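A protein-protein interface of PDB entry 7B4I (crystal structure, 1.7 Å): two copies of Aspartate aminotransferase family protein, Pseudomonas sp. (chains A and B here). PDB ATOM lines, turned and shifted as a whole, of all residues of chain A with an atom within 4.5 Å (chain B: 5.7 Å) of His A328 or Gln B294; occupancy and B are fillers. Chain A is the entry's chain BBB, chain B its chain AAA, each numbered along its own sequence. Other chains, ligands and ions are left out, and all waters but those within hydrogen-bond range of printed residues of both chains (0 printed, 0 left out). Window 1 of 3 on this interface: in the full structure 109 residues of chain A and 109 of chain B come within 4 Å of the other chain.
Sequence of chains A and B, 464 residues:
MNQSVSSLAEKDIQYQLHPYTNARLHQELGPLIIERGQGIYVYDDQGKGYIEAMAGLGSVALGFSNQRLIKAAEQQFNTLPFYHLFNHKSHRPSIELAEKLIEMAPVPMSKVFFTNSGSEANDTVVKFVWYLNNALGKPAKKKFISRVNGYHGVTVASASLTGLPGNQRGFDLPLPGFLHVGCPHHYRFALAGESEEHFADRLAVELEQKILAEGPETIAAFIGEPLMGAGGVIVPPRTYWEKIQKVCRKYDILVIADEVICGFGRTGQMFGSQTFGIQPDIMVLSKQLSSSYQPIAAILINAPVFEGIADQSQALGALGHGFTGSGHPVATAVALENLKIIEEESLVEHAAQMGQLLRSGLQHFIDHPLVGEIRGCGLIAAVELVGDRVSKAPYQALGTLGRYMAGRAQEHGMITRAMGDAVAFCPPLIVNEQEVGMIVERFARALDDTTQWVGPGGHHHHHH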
ATOM      1  N   PHE A  77       6.529 -31.270  31.318  1.00  0.00           N
ATOM      2  CA  PHE A  77       6.962 -30.154  32.196  1.00  0.00           C
ATOM      3  C   PHE A  77       7.321 -30.709  33.581  1.00  0.00           C
ATOM      4  O   PHE A  77       8.345 -30.351  34.158  1.00  0.00           O
ATOM      5  CB  PHE A  77       5.877 -29.088  32.349  1.00  0.00           C
ATOM      6  CG  PHE A  77       5.869 -28.006  31.308  1.00  0.00           C
ATOM      7  CD1 PHE A  77       7.000 -27.250  31.051  1.00  0.00           C
ATOM      8  CD2 PHE A  77       4.702 -27.705  30.621  1.00  0.00           C
ATOM      9  CE1 PHE A  77       6.967 -26.235  30.111  1.00  0.00           C
ATOM     10  CE2 PHE A  77       4.675 -26.691  29.678  1.00  0.00           C
ATOM     11  CZ  PHE A  77       5.809 -25.960  29.427  1.00  0.00           C
ATOM     12  N   PRO A  81      11.491 -30.133  32.142  1.00  0.00           N
ATOM     13  CA  PRO A  81      10.897 -29.036  31.385  1.00  0.00           C
ATOM     14  C   PRO A  81      11.840 -28.440  30.326  1.00  0.00           C
ATOM     15  O   PRO A  81      11.377 -27.728  29.436  1.00  0.00           O
ATOM     16  CB  PRO A  81      10.549 -28.001  32.457  1.00  0.00           C
ATOM     17  CG  PRO A  81      11.553 -28.250  33.561  1.00  0.00           C
ATOM     18  CD  PRO A  81      11.797 -29.741  33.536  1.00  0.00           C
ATOM     19  N   PHE A  82      13.128 -28.690  30.483  1.00  0.00           N
ATOM     20  CA  PHE A  82      14.155 -28.328  29.467  1.00  0.00           C
ATOM     21  C   PHE A  82      15.327 -29.287  29.580  1.00  0.00           C
ATOM     22  O   PHE A  82      15.782 -29.593  30.684  1.00  0.00           O
ATOM     23  CB  PHE A  82      14.678 -26.896  29.629  1.00  0.00           C
ATOM     24  CG  PHE A  82      15.809 -26.590  28.679  1.00  0.00           C
ATOM     25  CD1 PHE A  82      15.537 -26.357  27.342  1.00  0.00           C
ATOM     26  CD2 PHE A  82      17.130 -26.686  29.089  1.00  0.00           C
ATOM     27  CE1 PHE A  82      16.576 -26.129  26.444  1.00  0.00           C
ATOM     28  CE2 PHE A  82      18.165 -26.464  28.185  1.00  0.00           C
ATOM     29  CZ  PHE A  82      17.872 -26.188  26.872  1.00  0.00           C
ATOM     30  N   HIS A  91      17.273 -37.121  25.364  1.00  0.00           N
ATOM     31  CA  HIS A  91      16.076 -37.319  26.199  1.00  0.00           C
ATOM     32  C   HIS A  91      15.030 -38.067  25.395  1.00  0.00           C
ATOM     33  O   HIS A  91      15.092 -38.039  24.145  1.00  0.00           O
ATOM     34  CB  HIS A  91      15.600 -35.993  26.781  1.00  0.00           C
ATOM     35  CG  HIS A  91      15.303 -34.958  25.754  1.00  0.00           C
ATOM     36  ND1 HIS A  91      14.180 -35.043  24.947  1.00  0.00           N
ATOM     37  CD2 HIS A  91      15.926 -33.801  25.444  1.00  0.00           C
ATOM     38  CE1 HIS A  91      14.124 -33.969  24.195  1.00  0.00           C
ATOM     39  NE2 HIS A  91      15.181 -33.206  24.465  1.00  0.00           N
ATOM     40  N   GLN A 294       3.451 -25.918  20.168  1.00  0.00           N
ATOM     41  CA  GLN A 294       4.838 -25.638  20.579  1.00  0.00           C
ATOM     42  C   GLN A 294       5.654 -25.325  19.337  1.00  0.00           C
ATOM     43  O   GLN A 294       5.444 -25.939  18.304  1.00  0.00           O
ATOM     44  CB  GLN A 294       5.437 -26.856  21.268  1.00  0.00           C
ATOM     45  CG  GLN A 294       4.786 -27.159  22.617  1.00  0.00           C
ATOM     46  CD  GLN A 294       5.287 -26.204  23.655  1.00  0.00           C
ATOM     47  OE1 GLN A 294       6.366 -26.407  24.195  1.00  0.00           O
ATOM     48  NE2 GLN A 294       4.569 -25.111  23.868  1.00  0.00           N
ATOM     49  N   GLY A 325      17.066 -24.633  21.802  1.00  0.00           N
ATOM     50  CA  GLY A 325      15.756 -25.302  21.788  1.00  0.00           C
ATOM     51  C   GLY A 325      15.690 -26.529  20.889  1.00  0.00           C
ATOM     52  O   GLY A 325      14.593 -27.093  20.820  1.00  0.00           O
ATOM     53  N   SER A 326      16.750 -26.884  20.167  1.00  0.00           N
ATOM     54  CA  SER A 326      16.766 -28.075  19.272  1.00  0.00           C
ATOM     55  C   SER A 326      16.270 -29.287  20.059  1.00  0.00           C
ATOM     56  O   SER A 326      16.943 -29.701  21.004  1.00  0.00           O
ATOM     57  CB  SER A 326      18.121 -28.338  18.670  1.00  0.00           C
ATOM     58  OG  SER A 326      18.385 -27.469  17.574  1.00  0.00           O
ATOM     59  N   GLY A 327      15.126 -29.832  19.681  1.00  0.00           N
ATOM     60  CA  GLY A 327      14.571 -31.062  20.264  1.00  0.00           C
ATOM     61  C   GLY A 327      13.968 -30.822  21.637  1.00  0.00           C
ATOM     62  O   GLY A 327      13.754 -31.815  22.336  1.00  0.00           O
ATOM     63  N   HIS A 328      13.625 -29.570  21.957  1.00  0.00           N
ATOM     64  CA  HIS A 328      13.072 -29.189  23.281  1.00  0.00           C
ATOM     65  C   HIS A 328      12.114 -30.272  23.788  1.00  0.00           C
ATOM     66  O   HIS A 328      11.179 -30.635  23.096  1.00  0.00           O
ATOM     67  CB  HIS A 328      12.351 -27.852  23.179  1.00  0.00           C
ATOM     68  CG  HIS A 328      12.048 -27.278  24.515  1.00  0.00           C
ATOM     69  ND1 HIS A 328      11.013 -27.768  25.305  1.00  0.00           N
ATOM     70  CD2 HIS A 328      12.598 -26.242  25.184  1.00  0.00           C
ATOM     71  CE1 HIS A 328      10.987 -27.071  26.426  1.00  0.00           C
ATOM     72  NE2 HIS A 328      11.945 -26.137  26.383  1.00  0.00           N
ATOM     73  N   PRO A 329      12.288 -30.804  25.021  1.00  0.00           N
ATOM     74  CA  PRO A 329      11.511 -31.965  25.467  1.00  0.00           C
ATOM     75  C   PRO A 329      10.002 -31.722  25.508  1.00  0.00           C
ATOM     76  O   PRO A 329       9.246 -32.669  25.238  1.00  0.00           O
ATOM     77  CB  PRO A 329      12.071 -32.300  26.865  1.00  0.00           C
ATOM     78  CG  PRO A 329      12.835 -31.064  27.281  1.00  0.00           C
ATOM     79  CD  PRO A 329      13.312 -30.416  26.000  1.00  0.00           C
ATOM     80  N   VAL A 330       9.567 -30.509  25.844  1.00  0.00           N
ATOM     81  CA  VAL A 330       8.108 -30.213  25.861  1.00  0.00           C
ATOM     82  C   VAL A 330       7.607 -30.131  24.413  1.00  0.00           C
ATOM     83  O   VAL A 330       6.564 -30.679  24.119  1.00  0.00           O
ATOM     84  CB  VAL A 330       7.779 -28.962  26.687  1.00  0.00           C
ATOM     85  CG1 VAL A 330       6.282 -28.664  26.686  1.00  0.00           C
ATOM     86  CG2 VAL A 330       8.303 -29.123  28.110  1.00  0.00           C
ATOM     87  N   ALA A 331       8.348 -29.493  23.514  1.00  0.00           N
ATOM     88  CA  ALA A 331       7.906 -29.366  22.104  1.00  0.00           C
ATOM     89  C   ALA A 331       7.870 -30.753  21.454  1.00  0.00           C
ATOM     90  O   ALA A 331       6.909 -31.055  20.729  1.00  0.00           O
ATOM     91  CB  ALA A 331       8.805 -28.405  21.363  1.00  0.00           C
ATOM     92  N   THR A 332       8.891 -31.579  21.675  1.00  0.00           N
ATOM     93  CA  THR A 332       8.974 -32.928  21.062  1.00  0.00           C
ATOM     94  C   THR A 332       7.889 -33.824  21.673  1.00  0.00           C
ATOM     95  O   THR A 332       7.305 -34.623  20.933  1.00  0.00           O
ATOM     96  CB  THR A 332      10.370 -33.539  21.145  1.00  0.00           C
ATOM     97  OG1 THR A 332      10.858 -33.481  22.480  1.00  0.00           O
ATOM     98  CG2 THR A 332      11.348 -32.839  20.224  1.00  0.00           C
ATOM     99  N   PHE B  77      -2.498 -22.705  27.705  1.00  0.00           N
ATOM    100  CA  PHE B  77      -2.904 -23.823  26.818  1.00  0.00           C
ATOM    101  C   PHE B  77      -4.430 -23.921  26.800  1.00  0.00           C
ATOM    102  O   PHE B  77      -5.026 -24.084  25.733  1.00  0.00           O
ATOM    103  CB  PHE B  77      -2.320 -25.166  27.243  1.00  0.00           C
ATOM    104  CG  PHE B  77      -0.938 -25.485  26.715  1.00  0.00           C
ATOM    105  CD1 PHE B  77      -0.674 -25.495  25.349  1.00  0.00           C
ATOM    106  CD2 PHE B  77       0.083 -25.850  27.578  1.00  0.00           C
ATOM    107  CE1 PHE B  77       0.588 -25.815  24.872  1.00  0.00           C
ATOM    108  CE2 PHE B  77       1.345 -26.176  27.099  1.00  0.00           C
ATOM    109  CZ  PHE B  77       1.588 -26.171  25.744  1.00  0.00           C
ATOM    110  N   SER B 290      12.788 -17.263  29.704  1.00  0.00           N
ATOM    111  CA  SER B 290      11.724 -18.255  30.003  1.00  0.00           C
ATOM    112  C   SER B 290      12.264 -19.398  30.863  1.00  0.00           C
ATOM    113  O   SER B 290      11.568 -20.409  31.004  1.00  0.00           O
ATOM    114  CB  SER B 290      11.109 -18.796  28.736  1.00  0.00           C
ATOM    115  OG  SER B 290      12.068 -19.582  28.051  1.00  0.00           O
ATOM    116  N   SER B 291      13.463 -19.259  31.433  1.00  0.00           N
ATOM    117  CA  SER B 291      14.236 -20.375  32.041  1.00  0.00           C
ATOM    118  C   SER B 291      14.361 -21.525  31.040  1.00  0.00           C
ATOM    119  O   SER B 291      14.539 -22.674  31.466  1.00  0.00           O
ATOM    120  CB  SER B 291      13.637 -20.846  33.355  1.00  0.00           C
ATOM    121  OG  SER B 291      13.883 -19.888  34.364  1.00  0.00           O
ATOM    122  N   SER B 292      14.312 -21.212  29.740  1.00  0.00           N
ATOM    123  CA  SER B 292      14.312 -22.219  28.640  1.00  0.00           C
ATOM    124  C   SER B 292      13.136 -23.198  28.771  1.00  0.00           C
ATOM    125  O   SER B 292      13.159 -24.203  28.063  1.00  0.00           O
ATOM    126  CB  SER B 292      15.632 -22.966  28.565  1.00  0.00           C
ATOM    127  OG  SER B 292      16.603 -22.178  27.916  1.00  0.00           O
ATOM    128  N   TYR B 293      12.094 -22.914  29.568  1.00  0.00           N
ATOM    129  CA  TYR B 293      10.906 -23.808  29.640  1.00  0.00           C
ATOM    130  C   TYR B 293      10.157 -23.769  28.307  1.00  0.00           C
ATOM    131  O   TYR B 293       9.419 -24.706  28.007  1.00  0.00           O
ATOM    132  CB  TYR B 293       9.970 -23.422  30.786  1.00  0.00           C
ATOM    133  CG  TYR B 293      10.348 -23.996  32.130  1.00  0.00           C
ATOM    134  CD1 TYR B 293      11.660 -24.025  32.568  1.00  0.00           C
ATOM    135  CD2 TYR B 293       9.369 -24.493  32.981  1.00  0.00           C
ATOM    136  CE1 TYR B 293      11.998 -24.529  33.817  1.00  0.00           C
ATOM    137  CE2 TYR B 293       9.688 -24.999  34.232  1.00  0.00           C
ATOM    138  CZ  TYR B 293      11.005 -25.009  34.660  1.00  0.00           C
ATOM    139  OH  TYR B 293      11.361 -25.499  35.886  1.00  0.00           O
ATOM    140  N   GLN B 294      10.334 -22.688  27.554  1.00  0.00           N
ATOM    141  CA  GLN B 294       9.738 -22.498  26.216  1.00  0.00           C
ATOM    142  C   GLN B 294      10.755 -21.792  25.337  1.00  0.00           C
ATOM    143  O   GLN B 294      11.471 -20.916  25.797  1.00  0.00           O
ATOM    144  CB  GLN B 294       8.464 -21.663  26.287  1.00  0.00           C
ATOM    145  CG  GLN B 294       7.344 -22.358  27.041  1.00  0.00           C
ATOM    146  CD  GLN B 294       6.681 -23.381  26.167  1.00  0.00           C
ATOM    147  OE1 GLN B 294       5.839 -23.050  25.332  1.00  0.00           O
ATOM    148  NE2 GLN B 294       7.141 -24.603  26.278  1.00  0.00           N
ATOM    149  N   PRO B 295      10.827 -22.144  24.039  1.00  0.00           N
ATOM    150  CA  PRO B 295      11.691 -21.416  23.113  1.00  0.00           C
ATOM    151  C   PRO B 295      11.119 -20.017  22.843  1.00  0.00           C
ATOM    152  O   PRO B 295      10.066 -19.881  22.252  1.00  0.00           O
ATOM    153  CB  PRO B 295      11.627 -22.235  21.826  1.00  0.00           C
ATOM    154  CG  PRO B 295      11.079 -23.560  22.232  1.00  0.00           C
ATOM    155  CD  PRO B 295      10.168 -23.300  23.415  1.00  0.00           C
ATOM    156  N   ILE B 296      11.836 -18.999  23.279  1.00  0.00           N
ATOM    157  CA  ILE B 296      11.450 -17.602  22.988  1.00  0.00           C
ATOM    158  C   ILE B 296      12.695 -16.725  23.099  1.00  0.00           C
ATOM    159  O   ILE B 296      13.551 -16.966  23.991  1.00  0.00           O
ATOM    160  CB  ILE B 296      10.310 -17.125  23.912  1.00  0.00           C
ATOM    161  CG1 ILE B 296       9.946 -15.664  23.636  1.00  0.00           C
ATOM    162  CG2 ILE B 296      10.655 -17.366  25.373  1.00  0.00           C
ATOM    163  CD1 ILE B 296       8.655 -15.243  24.293  1.00  0.00           C
ATOM    164  N   HIS B 328       4.647 -16.519  20.527  1.00  0.00           N
ATOM    165  CA  HIS B 328       3.771 -17.678  20.799  1.00  0.00           C
ATOM    166  C   HIS B 328       3.101 -17.488  22.160  1.00  0.00           C
ATOM    167  O   HIS B 328       3.784 -17.253  23.156  1.00  0.00           O
ATOM    168  CB  HIS B 328       4.609 -18.961  20.798  1.00  0.00           C
ATOM    169  CG  HIS B 328       3.770 -20.192  20.824  1.00  0.00           C
ATOM    170  ND1 HIS B 328       3.085 -20.607  21.959  1.00  0.00           N
ATOM    171  CD2 HIS B 328       3.489 -21.096  19.860  1.00  0.00           C
ATOM    172  CE1 HIS B 328       2.432 -21.714  21.687  1.00  0.00           C
ATOM    173  NE2 HIS B 328       2.648 -22.031  20.403  1.00  0.00           N
ATOM    174  N   VAL B 330       1.871 -19.372  24.543  1.00  0.00           N
ATOM    175  CA  VAL B 330       2.346 -20.205  25.672  1.00  0.00           C
ATOM    176  C   VAL B 330       3.766 -19.773  26.041  1.00  0.00           C
ATOM    177  O   VAL B 330       4.063 -19.649  27.232  1.00  0.00           O
ATOM    178  CB  VAL B 330       2.221 -21.708  25.379  1.00  0.00           C
ATOM    179  CG1 VAL B 330       2.702 -22.543  26.547  1.00  0.00           C
ATOM    180  CG2 VAL B 330       0.790 -22.075  25.029  1.00  0.00           C
ATOM    181  N   ALA B 331       4.634 -19.521  25.071  1.00  0.00           N
ATOM    182  CA  ALA B 331       6.024 -19.114  25.362  1.00  0.00           C
ATOM    183  C   ALA B 331       6.019 -17.737  26.057  1.00  0.00           C
ATOM    184  O   ALA B 331       6.772 -17.552  27.028  1.00  0.00           O
ATOM    185  CB  ALA B 331       6.862 -19.105  24.116  1.00  0.00           C
ATOM    186  N   VAL B 334       4.695 -18.016  29.671  1.00  0.00           N
ATOM    187  CA  VAL B 334       5.722 -18.630  30.550  1.00  0.00           C
ATOM    188  C   VAL B 334       6.802 -17.586  30.842  1.00  0.00           C
ATOM    189  O   VAL B 334       7.216 -17.477  32.026  1.00  0.00           O
ATOM    190  CB  VAL B 334       6.300 -19.931  29.969  1.00  0.00           C
ATOM    191  CG1 VAL B 334       7.553 -20.355  30.709  1.00  0.00           C
ATOM    192  CG2 VAL B 334       5.264 -21.041  29.992  1.00  0.00           C
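Among the printed residues, merely in contact across the chains: Phe A82 with Ser B292 (3.3 Å), Pro A81 with Tyr B293 (3.5 Å), Phe A77 with Tyr B293 (3.6 Å), Gln A294 with Phe B77 (3.7 Å), Phe A77 with Gln B294 (3.7 Å), Gln A294 with His B328 (3.98 Å) and His A328 with Gln B294 (3.98 Å).
Of the printed residues of chain B, Phe A77 touches Tyr B293 (3.6 Å) and Gln B294 (3.7 Å). Printed residues of chain B within 4 Å of Pro A81: Tyr B293. Of the printed residues of chain B, His A328 touches Ser B292, Tyr B293 and Gln B294. Ala A331 touches none of the printed residues of chain B. Of the printed residues of chain A, Tyr B293 touches Phe A77 (3.6 Å), Pro A81 (3.5 Å) and His A328 (3.2 Å). Of the printed residues of chain A, Gln B294 touches Phe A77, Gln A294 and His A328. Printed residues of chain A within 4 Å of His B328: Gln A294 (3.98 Å). The nearest printed residue of chain B that does not touch His A328 is Pro B295 (4.2 Å). The nearest printed residue of chain A that does not touch Gln B294 is Val A330 (4.2 Å).
The side-chain hydroxyl of Ser B290 sits close to the backbone NH of Ser B292. O of Gln B294 lies within hydrogen-bond range of OG of Ser B290 (2.7 Å). ND1 of His B328 sits at hydrogen-bond distance from N of Val B330 (3.1 Å). The backbone carbonyl oxygen (O) of Pro A81 lies close to a ring nitrogen (NE2) of His A328 (3.5 Å). ND1 of His A328 lies within hydrogen-bond range of N of Val A330 (3.1 Å). O of His A328 lies within hydrogen-bond range of OG1 of Thr A332.
Hydrophobic or aromatic side chains of chain A that line the printed part of chain B: Phe A77, Pro A81, Phe A82 and His A328. Hydrophobic or aromatic side chains of chain B that line the printed part of chain A: Phe B77, Tyr B293 and His B328.
A ring nitrogen (NE2) of His A328 lies within hydrogen-bond range of the backbone carbonyl oxygen (O) of Ser B292 (2.8 Å). A ring nitrogen (NE2) of His A328 lies close to the backbone carbonyl oxygen of Tyr B293, 3.3 Å away. OE1 of Gln B294 lies within hydrogen-bond range of NE2 of Gln A294, at 2.8 Å.
Phe A77 touches Gln B294, and with the chains exchanged Gln A294 touches Phe B77. Gln A294 touches its own counterpart, Gln B294. Gln A294 touches His B328, and with the chains exchanged His A328 touches Gln B294. 5 positions are printed for both chains.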
